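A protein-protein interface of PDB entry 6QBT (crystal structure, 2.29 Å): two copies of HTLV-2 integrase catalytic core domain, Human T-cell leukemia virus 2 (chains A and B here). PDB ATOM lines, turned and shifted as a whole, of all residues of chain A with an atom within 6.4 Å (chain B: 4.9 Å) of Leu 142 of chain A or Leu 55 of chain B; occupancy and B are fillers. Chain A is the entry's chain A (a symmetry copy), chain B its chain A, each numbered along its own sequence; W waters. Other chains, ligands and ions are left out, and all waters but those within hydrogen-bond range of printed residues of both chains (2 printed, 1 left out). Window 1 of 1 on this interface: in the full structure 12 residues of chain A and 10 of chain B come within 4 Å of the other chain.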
ATOM      1  N   TYR A 119       1.355  21.016 -18.959  1.00  0.00           N
ATOM      2  CA  TYR A 119      -0.066  21.317 -19.154  1.00  0.00           C
ATOM      3  C   TYR A 119      -0.331  22.392 -20.232  1.00  0.00           C
ATOM      4  O   TYR A 119      -1.353  22.331 -20.927  1.00  0.00           O
ATOM      5  CB  TYR A 119      -0.754  21.677 -17.818  1.00  0.00           C
ATOM      6  CG  TYR A 119      -1.029  20.462 -16.949  1.00  0.00           C
ATOM      7  CD1 TYR A 119      -1.873  19.427 -17.392  1.00  0.00           C
ATOM      8  CD2 TYR A 119      -0.454  20.344 -15.680  1.00  0.00           C
ATOM      9  CE1 TYR A 119      -2.118  18.312 -16.599  1.00  0.00           C
ATOM     10  CE2 TYR A 119      -0.689  19.230 -14.886  1.00  0.00           C
ATOM     11  CZ  TYR A 119      -1.517  18.220 -15.349  1.00  0.00           C
ATOM     12  OH  TYR A 119      -1.728  17.131 -14.539  1.00  0.00           O
ATOM     13  N   ASN A 133      -3.509  25.721 -12.206  1.00  0.00           N
ATOM     14  CA  ASN A 133      -4.410  24.991 -11.305  1.00  0.00           C
ATOM     15  C   ASN A 133      -4.127  23.483 -11.363  1.00  0.00           C
ATOM     16  O   ASN A 133      -3.942  22.818 -10.332  1.00  0.00           O
ATOM     17  CB  ASN A 133      -5.875  25.274 -11.632  1.00  0.00           C
ATOM     18  CG  ASN A 133      -6.781  24.979 -10.475  1.00  0.00           C
ATOM     19  OD1 ASN A 133      -6.529  25.405  -9.356  1.00  0.00           O
ATOM     20  ND2 ASN A 133      -7.816  24.220 -10.716  1.00  0.00           N
ATOM     21  N   LYS A 134      -4.051  22.961 -12.572  1.00  0.00           N
ATOM     22  CA  LYS A 134      -3.817  21.544 -12.756  1.00  0.00           C
ATOM     23  C   LYS A 134      -2.409  21.158 -12.285  1.00  0.00           C
ATOM     24  O   LYS A 134      -2.233  20.108 -11.693  1.00  0.00           O
ATOM     25  CB  LYS A 134      -4.052  21.156 -14.193  1.00  0.00           C
ATOM     26  CG  LYS A 134      -5.508  21.296 -14.585  1.00  0.00           C
ATOM     27  CD  LYS A 134      -5.706  20.860 -16.023  1.00  0.00           C
ATOM     28  CE  LYS A 134      -5.076  21.837 -17.009  1.00  0.00           C
ATOM     29  NZ  LYS A 134      -5.539  21.559 -18.382  1.00  0.00           N
ATOM     30  N   ALA A 135      -1.431  22.042 -12.467  1.00  0.00           N
ATOM     31  CA  ALA A 135      -0.093  21.816 -11.895  1.00  0.00           C
ATOM     32  C   ALA A 135      -0.170  21.694 -10.383  1.00  0.00           C
ATOM     33  O   ALA A 135       0.362  20.733  -9.810  1.00  0.00           O
ATOM     34  CB  ALA A 135       0.888  22.914 -12.295  1.00  0.00           C
ATOM     35  N   TRP A 137      -2.808  21.057  -8.249  1.00  0.00           N
ATOM     36  CA  TRP A 137      -3.523  19.890  -7.755  1.00  0.00           C
ATOM     37  C   TRP A 137      -2.805  18.579  -8.088  1.00  0.00           C
ATOM     38  O   TRP A 137      -2.775  17.654  -7.256  1.00  0.00           O
ATOM     39  CB  TRP A 137      -4.975  19.897  -8.244  1.00  0.00           C
ATOM     40  CG  TRP A 137      -5.755  20.915  -7.509  1.00  0.00           C
ATOM     41  CD1 TRP A 137      -5.974  22.205  -7.873  1.00  0.00           C
ATOM     42  CD2 TRP A 137      -6.392  20.739  -6.255  1.00  0.00           C
ATOM     43  NE1 TRP A 137      -6.737  22.850  -6.921  1.00  0.00           N
ATOM     44  CE2 TRP A 137      -6.991  21.976  -5.904  1.00  0.00           C
ATOM     45  CE3 TRP A 137      -6.511  19.660  -5.385  1.00  0.00           C
ATOM     46  CZ2 TRP A 137      -7.706  22.159  -4.719  1.00  0.00           C
ATOM     47  CZ3 TRP A 137      -7.208  19.827  -4.216  1.00  0.00           C
ATOM     48  CH2 TRP A 137      -7.812  21.076  -3.894  1.00  0.00           C
ATOM     49  N   THR A 138      -2.208  18.508  -9.269  1.00  0.00           N
ATOM     50  CA  THR A 138      -1.415  17.354  -9.650  1.00  0.00           C
ATOM     51  C   THR A 138      -0.248  17.152  -8.667  1.00  0.00           C
ATOM     52  O   THR A 138      -0.016  16.033  -8.190  1.00  0.00           O
ATOM     53  CB  THR A 138      -0.883  17.463 -11.105  1.00  0.00           C
ATOM     54  OG1 THR A 138      -1.985  17.484 -12.033  1.00  0.00           O
ATOM     55  CG2 THR A 138       0.032  16.262 -11.459  1.00  0.00           C
ATOM     56  N   LEU A 139       0.490  18.211  -8.356  1.00  0.00           N
ATOM     57  CA  LEU A 139       1.626  18.047  -7.463  1.00  0.00           C
ATOM     58  C   LEU A 139       1.192  17.602  -6.045  1.00  0.00           C
ATOM     59  O   LEU A 139       1.808  16.696  -5.471  1.00  0.00           O
ATOM     60  CB  LEU A 139       2.444  19.336  -7.394  1.00  0.00           C
ATOM     61  CG  LEU A 139       3.702  19.328  -6.502  1.00  0.00           C
ATOM     62  CD1 LEU A 139       4.687  18.238  -6.904  1.00  0.00           C
ATOM     63  CD2 LEU A 139       4.365  20.685  -6.577  1.00  0.00           C
ATOM     64  N   ASN A 140       0.151  18.228  -5.497  1.00  0.00           N
ATOM     65  CA  ASN A 140      -0.288  17.928  -4.121  1.00  0.00           C
ATOM     66  C   ASN A 140      -0.944  16.562  -4.015  1.00  0.00           C
ATOM     67  O   ASN A 140      -0.628  15.806  -3.090  1.00  0.00           O
ATOM     68  CB  ASN A 140      -1.224  18.999  -3.543  1.00  0.00           C
ATOM     69  CG  ASN A 140      -0.487  20.258  -3.104  1.00  0.00           C
ATOM     70  OD1 ASN A 140       0.638  20.198  -2.569  1.00  0.00           O
ATOM     71  ND2 ASN A 140      -1.128  21.416  -3.283  1.00  0.00           N
ATOM     72  N   GLN A 141      -1.807  16.219  -4.973  1.00  0.00           N
ATOM     73  CA  GLN A 141      -2.674  15.044  -4.823  1.00  0.00           C
ATOM     74  C   GLN A 141      -2.322  13.813  -5.598  1.00  0.00           C
ATOM     75  O   GLN A 141      -2.734  12.708  -5.191  1.00  0.00           O
ATOM     76  CB  GLN A 141      -4.106  15.387  -5.200  1.00  0.00           C
ATOM     77  CG  GLN A 141      -4.861  16.084  -4.108  1.00  0.00           C
ATOM     78  CD  GLN A 141      -6.334  16.036  -4.419  1.00  0.00           C
ATOM     79  OE1 GLN A 141      -6.764  16.572  -5.455  1.00  0.00           O
ATOM     80  NE2 GLN A 141      -7.108  15.313  -3.574  1.00  0.00           N
ATOM     81  N   LEU A 142      -1.632  13.990  -6.724  1.00  0.00           N
ATOM     82  CA  LEU A 142      -1.327  12.878  -7.604  1.00  0.00           C
ATOM     83  C   LEU A 142       0.084  12.329  -7.390  1.00  0.00           C
ATOM     84  O   LEU A 142       0.307  11.108  -7.307  1.00  0.00           O
ATOM     85  CB  LEU A 142      -1.534  13.273  -9.075  1.00  0.00           C
ATOM     86  CG  LEU A 142      -2.973  13.247  -9.599  1.00  0.00           C
ATOM     87  CD1 LEU A 142      -3.556  11.862  -9.640  1.00  0.00           C
ATOM     88  CD2 LEU A 142      -3.860  14.166  -8.771  1.00  0.00           C
ATOM     89  N   ASN A 143       1.033  13.240  -7.323  1.00  0.00           N
ATOM     90  CA  ASN A 143       2.438  12.889  -7.194  1.00  0.00           C
ATOM     91  C   ASN A 143       2.740  12.074  -5.914  1.00  0.00           C
ATOM     92  O   ASN A 143       2.456  12.523  -4.782  1.00  0.00           O
ATOM     93  CB  ASN A 143       3.234  14.180  -7.202  1.00  0.00           C
ATOM     94  CG  ASN A 143       4.629  13.969  -7.618  1.00  0.00           C
ATOM     95  OD1 ASN A 143       4.969  14.206  -8.778  1.00  0.00           O
ATOM     96  ND2 ASN A 143       5.460  13.478  -6.694  1.00  0.00           N
ATOM     97  N   VAL A 144       3.268  10.861  -6.104  1.00  0.00           N
ATOM     98  CA  VAL A 144       3.726  10.028  -4.985  1.00  0.00           C
ATOM     99  C   VAL A 144       5.184  10.332  -4.631  1.00  0.00           C
ATOM    100  O   VAL A 144       6.069  10.243  -5.470  1.00  0.00           O
ATOM    101  CB  VAL A 144       3.553   8.530  -5.262  1.00  0.00           C
ATOM    102  CG1 VAL A 144       3.959   7.720  -4.027  1.00  0.00           C
ATOM    103  CG2 VAL A 144       2.089   8.250  -5.593  1.00  0.00           C
ATOM    104  N   THR A 151       1.350  10.977  -0.988  1.00  0.00           N
ATOM    105  CA  THR A 151       1.271  12.233  -1.640  1.00  0.00           C
ATOM    106  C   THR A 151       1.383  13.294  -0.557  1.00  0.00           C
ATOM    107  O   THR A 151       1.157  13.012   0.622  1.00  0.00           O
ATOM    108  CB  THR A 151      -0.059  12.386  -2.382  1.00  0.00           C
ATOM    109  OG1 THR A 151      -1.124  12.403  -1.423  1.00  0.00           O
ATOM    110  CG2 THR A 151      -0.248  11.238  -3.346  1.00  0.00           C
ATOM    111  N   ILE B  51      -8.428  14.580 -18.693  1.00  0.00           N
ATOM    112  CA  ILE B  51      -7.481  14.698 -17.582  1.00  0.00           C
ATOM    113  C   ILE B  51      -7.909  15.828 -16.627  1.00  0.00           C
ATOM    114  O   ILE B  51      -7.849  15.672 -15.404  1.00  0.00           O
ATOM    115  CB  ILE B  51      -6.047  14.916 -18.116  1.00  0.00           C
ATOM    116  CG1 ILE B  51      -5.535  13.596 -18.703  1.00  0.00           C
ATOM    117  CG2 ILE B  51      -5.099  15.433 -17.026  1.00  0.00           C
ATOM    118  CD1 ILE B  51      -4.249  13.723 -19.481  1.00  0.00           C
ATOM    119  N   SER B  52      -8.299  16.972 -17.197  1.00  0.00           N
ATOM    120  CA  SER B  52      -8.833  18.082 -16.424  1.00  0.00           C
ATOM    121  C   SER B  52     -10.057  17.687 -15.549  1.00  0.00           C
ATOM    122  O   SER B  52     -10.056  17.977 -14.343  1.00  0.00           O
ATOM    123  CB  SER B  52      -9.187  19.257 -17.322  1.00  0.00           C
ATOM    124  OG  SER B  52      -9.676  20.358 -16.549  1.00  0.00           O
ATOM    125  N   ALA B  53     -11.061  17.018 -16.115  1.00  0.00           N
ATOM    126  CA  ALA B  53     -12.228  16.613 -15.297  1.00  0.00           C
ATOM    127  C   ALA B  53     -11.820  15.627 -14.228  1.00  0.00           C
ATOM    128  O   ALA B  53     -12.406  15.590 -13.158  1.00  0.00           O
ATOM    129  CB  ALA B  53     -13.318  15.987 -16.153  1.00  0.00           C
ATOM    130  N   PHE B  54     -10.838  14.797 -14.541  1.00  0.00           N
ATOM    131  CA  PHE B  54     -10.382  13.789 -13.611  1.00  0.00           C
ATOM    132  C   PHE B  54      -9.676  14.438 -12.420  1.00  0.00           C
ATOM    133  O   PHE B  54      -9.896  14.040 -11.272  1.00  0.00           O
ATOM    134  CB  PHE B  54      -9.498  12.776 -14.348  1.00  0.00           C
ATOM    135  CG  PHE B  54      -9.147  11.545 -13.561  1.00  0.00           C
ATOM    136  CD1 PHE B  54     -10.040  10.948 -12.664  1.00  0.00           C
ATOM    137  CD2 PHE B  54      -7.915  10.923 -13.778  1.00  0.00           C
ATOM    138  CE1 PHE B  54      -9.694   9.788 -11.981  1.00  0.00           C
ATOM    139  CE2 PHE B  54      -7.561   9.767 -13.089  1.00  0.00           C
ATOM    140  CZ  PHE B  54      -8.448   9.198 -12.193  1.00  0.00           C
ATOM    141  N   LEU B  55      -8.867  15.455 -12.690  1.00  0.00           N
ATOM    142  CA  LEU B  55      -8.291  16.305 -11.623  1.00  0.00           C
ATOM    143  C   LEU B  55      -9.351  17.058 -10.809  1.00  0.00           C
ATOM    144  O   LEU B  55      -9.201  17.159  -9.609  1.00  0.00           O
ATOM    145  CB  LEU B  55      -7.272  17.309 -12.162  1.00  0.00           C
ATOM    146  CG  LEU B  55      -5.987  16.662 -12.704  1.00  0.00           C
ATOM    147  CD1 LEU B  55      -5.207  17.621 -13.609  1.00  0.00           C
ATOM    148  CD2 LEU B  55      -5.106  16.169 -11.570  1.00  0.00           C
ATOM    149  N   GLN B  56     -10.387  17.602 -11.452  1.00  0.00           N
ATOM    150  CA  GLN B  56     -11.482  18.210 -10.703  1.00  0.00           C
ATOM    151  C   GLN B  56     -12.099  17.196  -9.739  1.00  0.00           C
ATOM    152  O   GLN B  56     -12.256  17.480  -8.559  1.00  0.00           O
ATOM    153  CB  GLN B  56     -12.531  18.797 -11.629  1.00  0.00           C
ATOM    154  CG  GLN B  56     -12.035  20.085 -12.260  1.00  0.00           C
ATOM    155  CD  GLN B  56     -12.845  20.569 -13.461  1.00  0.00           C
ATOM    156  OE1 GLN B  56     -13.586  19.812 -14.102  1.00  0.00           O
ATOM    157  NE2 GLN B  56     -12.685  21.845 -13.774  1.00  0.00           N
ATOM    158  N   ALA B  57     -12.414  16.014 -10.247  1.00  0.00           N
ATOM    159  CA  ALA B  57     -12.953  14.916  -9.434  1.00  0.00           C
ATOM    160  C   ALA B  57     -12.078  14.526  -8.225  1.00  0.00           C
ATOM    161  O   ALA B  57     -12.571  14.343  -7.091  1.00  0.00           O
ATOM    162  CB  ALA B  57     -13.162  13.703 -10.323  1.00  0.00           C
ATOM    163  N   ILE B  58     -10.788  14.379  -8.488  1.00  0.00           N
ATOM    164  CA  ILE B  58      -9.834  14.047  -7.452  1.00  0.00           C
ATOM    165  C   ILE B  58      -9.729  15.174  -6.433  1.00  0.00           C
ATOM    166  O   ILE B  58      -9.720  14.898  -5.238  1.00  0.00           O
ATOM    167  CB  ILE B  58      -8.477  13.671  -8.060  1.00  0.00           C
ATOM    168  CG1 ILE B  58      -8.614  12.297  -8.751  1.00  0.00           C
ATOM    169  CG2 ILE B  58      -7.388  13.649  -6.998  1.00  0.00           C
ATOM    170  CD1 ILE B  58      -7.501  11.974  -9.740  1.00  0.00           C
ATOM    171  N   SER B  59      -9.738  16.432  -6.863  1.00  0.00           N
ATOM    172  CA  SER B  59      -9.733  17.523  -5.875  1.00  0.00           C
ATOM    173  C   SER B  59     -10.943  17.503  -4.943  1.00  0.00           C
ATOM    174  O   SER B  59     -10.860  17.928  -3.815  1.00  0.00           O
ATOM    175  CB  SER B  59      -9.663  18.888  -6.538  1.00  0.00           C
ATOM    176  OG  SER B  59     -10.840  19.144  -7.282  1.00  0.00           O
ATOM    177  N   LYS B  63      -7.930  10.893  -4.171  1.00  0.00           N
ATOM    178  CA  LYS B  63      -7.330  10.071  -5.231  1.00  0.00           C
ATOM    179  C   LYS B  63      -7.823   8.619  -5.174  1.00  0.00           C
ATOM    180  O   LYS B  63      -7.665   7.980  -4.151  1.00  0.00           O
ATOM    181  CB  LYS B  63      -5.819  10.111  -5.065  1.00  0.00           C
ATOM    182  CG  LYS B  63      -5.018   9.343  -6.105  1.00  0.00           C
ATOM    183  CD  LYS B  63      -3.530   9.465  -5.828  1.00  0.00           C
ATOM    184  CE  LYS B  63      -2.733   8.835  -6.932  1.00  0.00           C
ATOM    185  NZ  LYS B  63      -1.281   8.882  -6.618  1.00  0.00           N
ATOM    186  N   PHE B  83      -0.879   9.304 -17.629  1.00  0.00           N
ATOM    187  CA  PHE B  83      -1.317   9.954 -16.411  1.00  0.00           C
ATOM    188  C   PHE B  83      -1.578   8.900 -15.341  1.00  0.00           C
ATOM    189  O   PHE B  83      -1.022   8.957 -14.251  1.00  0.00           O
ATOM    190  CB  PHE B  83      -2.557  10.821 -16.698  1.00  0.00           C
ATOM    191  CG  PHE B  83      -3.084  11.543 -15.498  1.00  0.00           C
ATOM    192  CD1 PHE B  83      -3.971  10.910 -14.618  1.00  0.00           C
ATOM    193  CD2 PHE B  83      -2.708  12.863 -15.238  1.00  0.00           C
ATOM    194  CE1 PHE B  83      -4.454  11.584 -13.501  1.00  0.00           C
ATOM    195  CE2 PHE B  83      -3.200  13.537 -14.127  1.00  0.00           C
ATOM    196  CZ  PHE B  83      -4.065  12.897 -13.254  1.00  0.00           C
ATOM    197  N   TYR B  87       0.911   8.205 -11.914  1.00  0.00           N
ATOM    198  CA  TYR B  87       0.382   8.467 -10.577  1.00  0.00           C
ATOM    199  C   TYR B  87      -0.246   7.253  -9.897  1.00  0.00           C
ATOM    200  O   TYR B  87      -0.939   7.426  -8.889  1.00  0.00           O
ATOM    201  CB  TYR B  87      -0.554   9.689 -10.619  1.00  0.00           C
ATOM    202  CG  TYR B  87       0.138  10.878 -11.249  1.00  0.00           C
ATOM    203  CD1 TYR B  87       1.297  11.409 -10.667  1.00  0.00           C
ATOM    204  CD2 TYR B  87      -0.355  11.463 -12.423  1.00  0.00           C
ATOM    205  CE1 TYR B  87       1.942  12.502 -11.231  1.00  0.00           C
ATOM    206  CE2 TYR B  87       0.282  12.545 -13.005  1.00  0.00           C
ATOM    207  CZ  TYR B  87       1.434  13.074 -12.414  1.00  0.00           C
ATOM    208  OH  TYR B  87       2.093  14.150 -13.012  1.00  0.00           O
ATOM    209  N   ILE B  89      -2.582   4.804 -10.627  1.00  0.00           N
ATOM    210  CA  ILE B  89      -4.012   4.595 -10.632  1.00  0.00           C
ATOM    211  C   ILE B  89      -4.274   3.432 -11.598  1.00  0.00           C
ATOM    212  O   ILE B  89      -3.969   3.533 -12.797  1.00  0.00           O
ATOM    213  CB  ILE B  89      -4.758   5.865 -11.091  1.00  0.00           C
ATOM    214  CG1 ILE B  89      -4.477   7.041 -10.138  1.00  0.00           C
ATOM    215  CG2 ILE B  89      -6.257   5.607 -11.128  1.00  0.00           C
ATOM    216  CD1 ILE B  89      -4.859   8.409 -10.680  1.00  0.00           C
HETATM  217  O   HOH W   1      -8.439  22.661 -17.822  1.00  0.00           O
HETATM  218  O   HOH W   2       3.983  15.038 -11.248  1.00  0.00           O
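O of Ile 58 of chain B sits at hydrogen-bond distance from NE2 of Gln 141 of chain A (3.1 Å).
The backbone NH of Ser 59 of chain B lies close to the side-chain amide oxygen of Gln 141 of chain A (3.3 Å).
The side-chain amino group of Lys 63 of chain B lies within hydrogen-bond range of the backbone carbonyl oxygen of Leu 142 of chain A (2.8 Å).
O of Leu 55 of chain B lies within hydrogen-bond range of OG of Ser 59 of chain B (3.5 Å).
The backbone carbonyl oxygen (O) of Gln 56 of chain B lies within hydrogen-bond range of the side-chain hydroxyl (OG) of Ser 59 of chain B (2.5 Å).
The backbone carbonyl oxygen of Tyr 87 of chain B sits at hydrogen-bond distance from the side-chain amino group of Lys 63 of chain B, 2.7 Å away.
The side-chain hydroxyl (OH) of Tyr 119 of chain A is in hydrogen-bond range of the side-chain hydroxyl (OG1) of Thr 138 of chain A, 2.5 Å away.
The backbone carbonyl oxygen (O) of Lys 134 of chain A is in hydrogen-bond range of the side-chain hydroxyl (OG1) of Thr 138 of chain A (2.7 Å).
The backbone carbonyl oxygen (O) of Thr 138 of chain A lies within hydrogen-bond range of the backbone NH (N) of Asn 143 of chain A (3.1 Å).
Among the printed residues, pairs that only touch across the chains: Thr 138 of chain A with Tyr 87 of chain B (3.3 Å), Gln 141 of chain A with Lys 63 of chain B (3.4 Å), Thr 138 of chain A with Leu 55 of chain B (3.4 Å), Trp 137 of chain A with Ser 59 of chain B (3.4 Å), Leu 142 of chain A with Tyr 87 of chain B (3.5 Å), Val 144 of chain A with Lys 63 of chain B (3.6 Å), Tyr 119 of chain A with Leu 55 of chain B (3.6 Å), Leu 142 of chain A with Leu 55 of chain B (3.7 Å), Lys 134 of chain A with Leu 55 of chain B (3.8 Å), Leu 142 of chain A with Phe 83 of chain B (3.8 Å), Asn 143 of chain A with Tyr 87 of chain B (3.8 Å), Leu 142 of chain A with Ile 89 of chain B (3.8 Å), Tyr 119 of chain A with Phe 83 of chain B (3.9 Å) and Leu 142 of chain A with Ile 58 of chain B (3.9 Å).
Ala 135 of chain A touches none of the printed residues of chain B.
Leu 139 of chain A touches none of the printed residues of chain B.
Printed residues of chain B within 4 Å of Gln 141 of chain A: Ile 58, Ser 59 and Lys 63.
Leu 142 of chain A touches just these residues of chain B: Leu 55 (3.7 Å), Ile 58 (3.9 Å), Lys 63 (2.8 Å), Phe 83 (3.8 Å), Tyr 87 (3.5 Å) and Ile 89 (3.8 Å).
Leu 55 of chain B touches just these residues of chain A: Tyr 119 (3.6 Å), Lys 134 (3.8 Å), Thr 138 (3.4 Å) and Leu 142 (3.7 Å).
Of the printed residues of chain A, Phe 83 of chain B touches Tyr 119 (3.9 Å) and Leu 142 (3.8 Å).
The nearest residue of chain A that does not touch Leu 55 of chain B is Trp 137 of chain A (4.8 Å).
Hydrophobic or aromatic side chains of chain A that line the printed part of chain B: Tyr 119, Trp 137, Leu 142 and Val 144.
Printed residues of chain B that touch a printed residue of chain A: Leu 55, Ile 58, Ser 59, Lys 63, Phe 83, Tyr 87 and Ile 89.
No position is printed for both chains.
Water W2 lies within hydrogen-bond range of OH of Tyr 87 of chain B (2.7 Å) and OD1 of Asn 143 of chain A (2.8 Å).
Water W1 lies within hydrogen-bond range of OG of Ser 52 of chain B (2.9 Å) and NZ of Lys 134 of chain A (3.2 Å).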
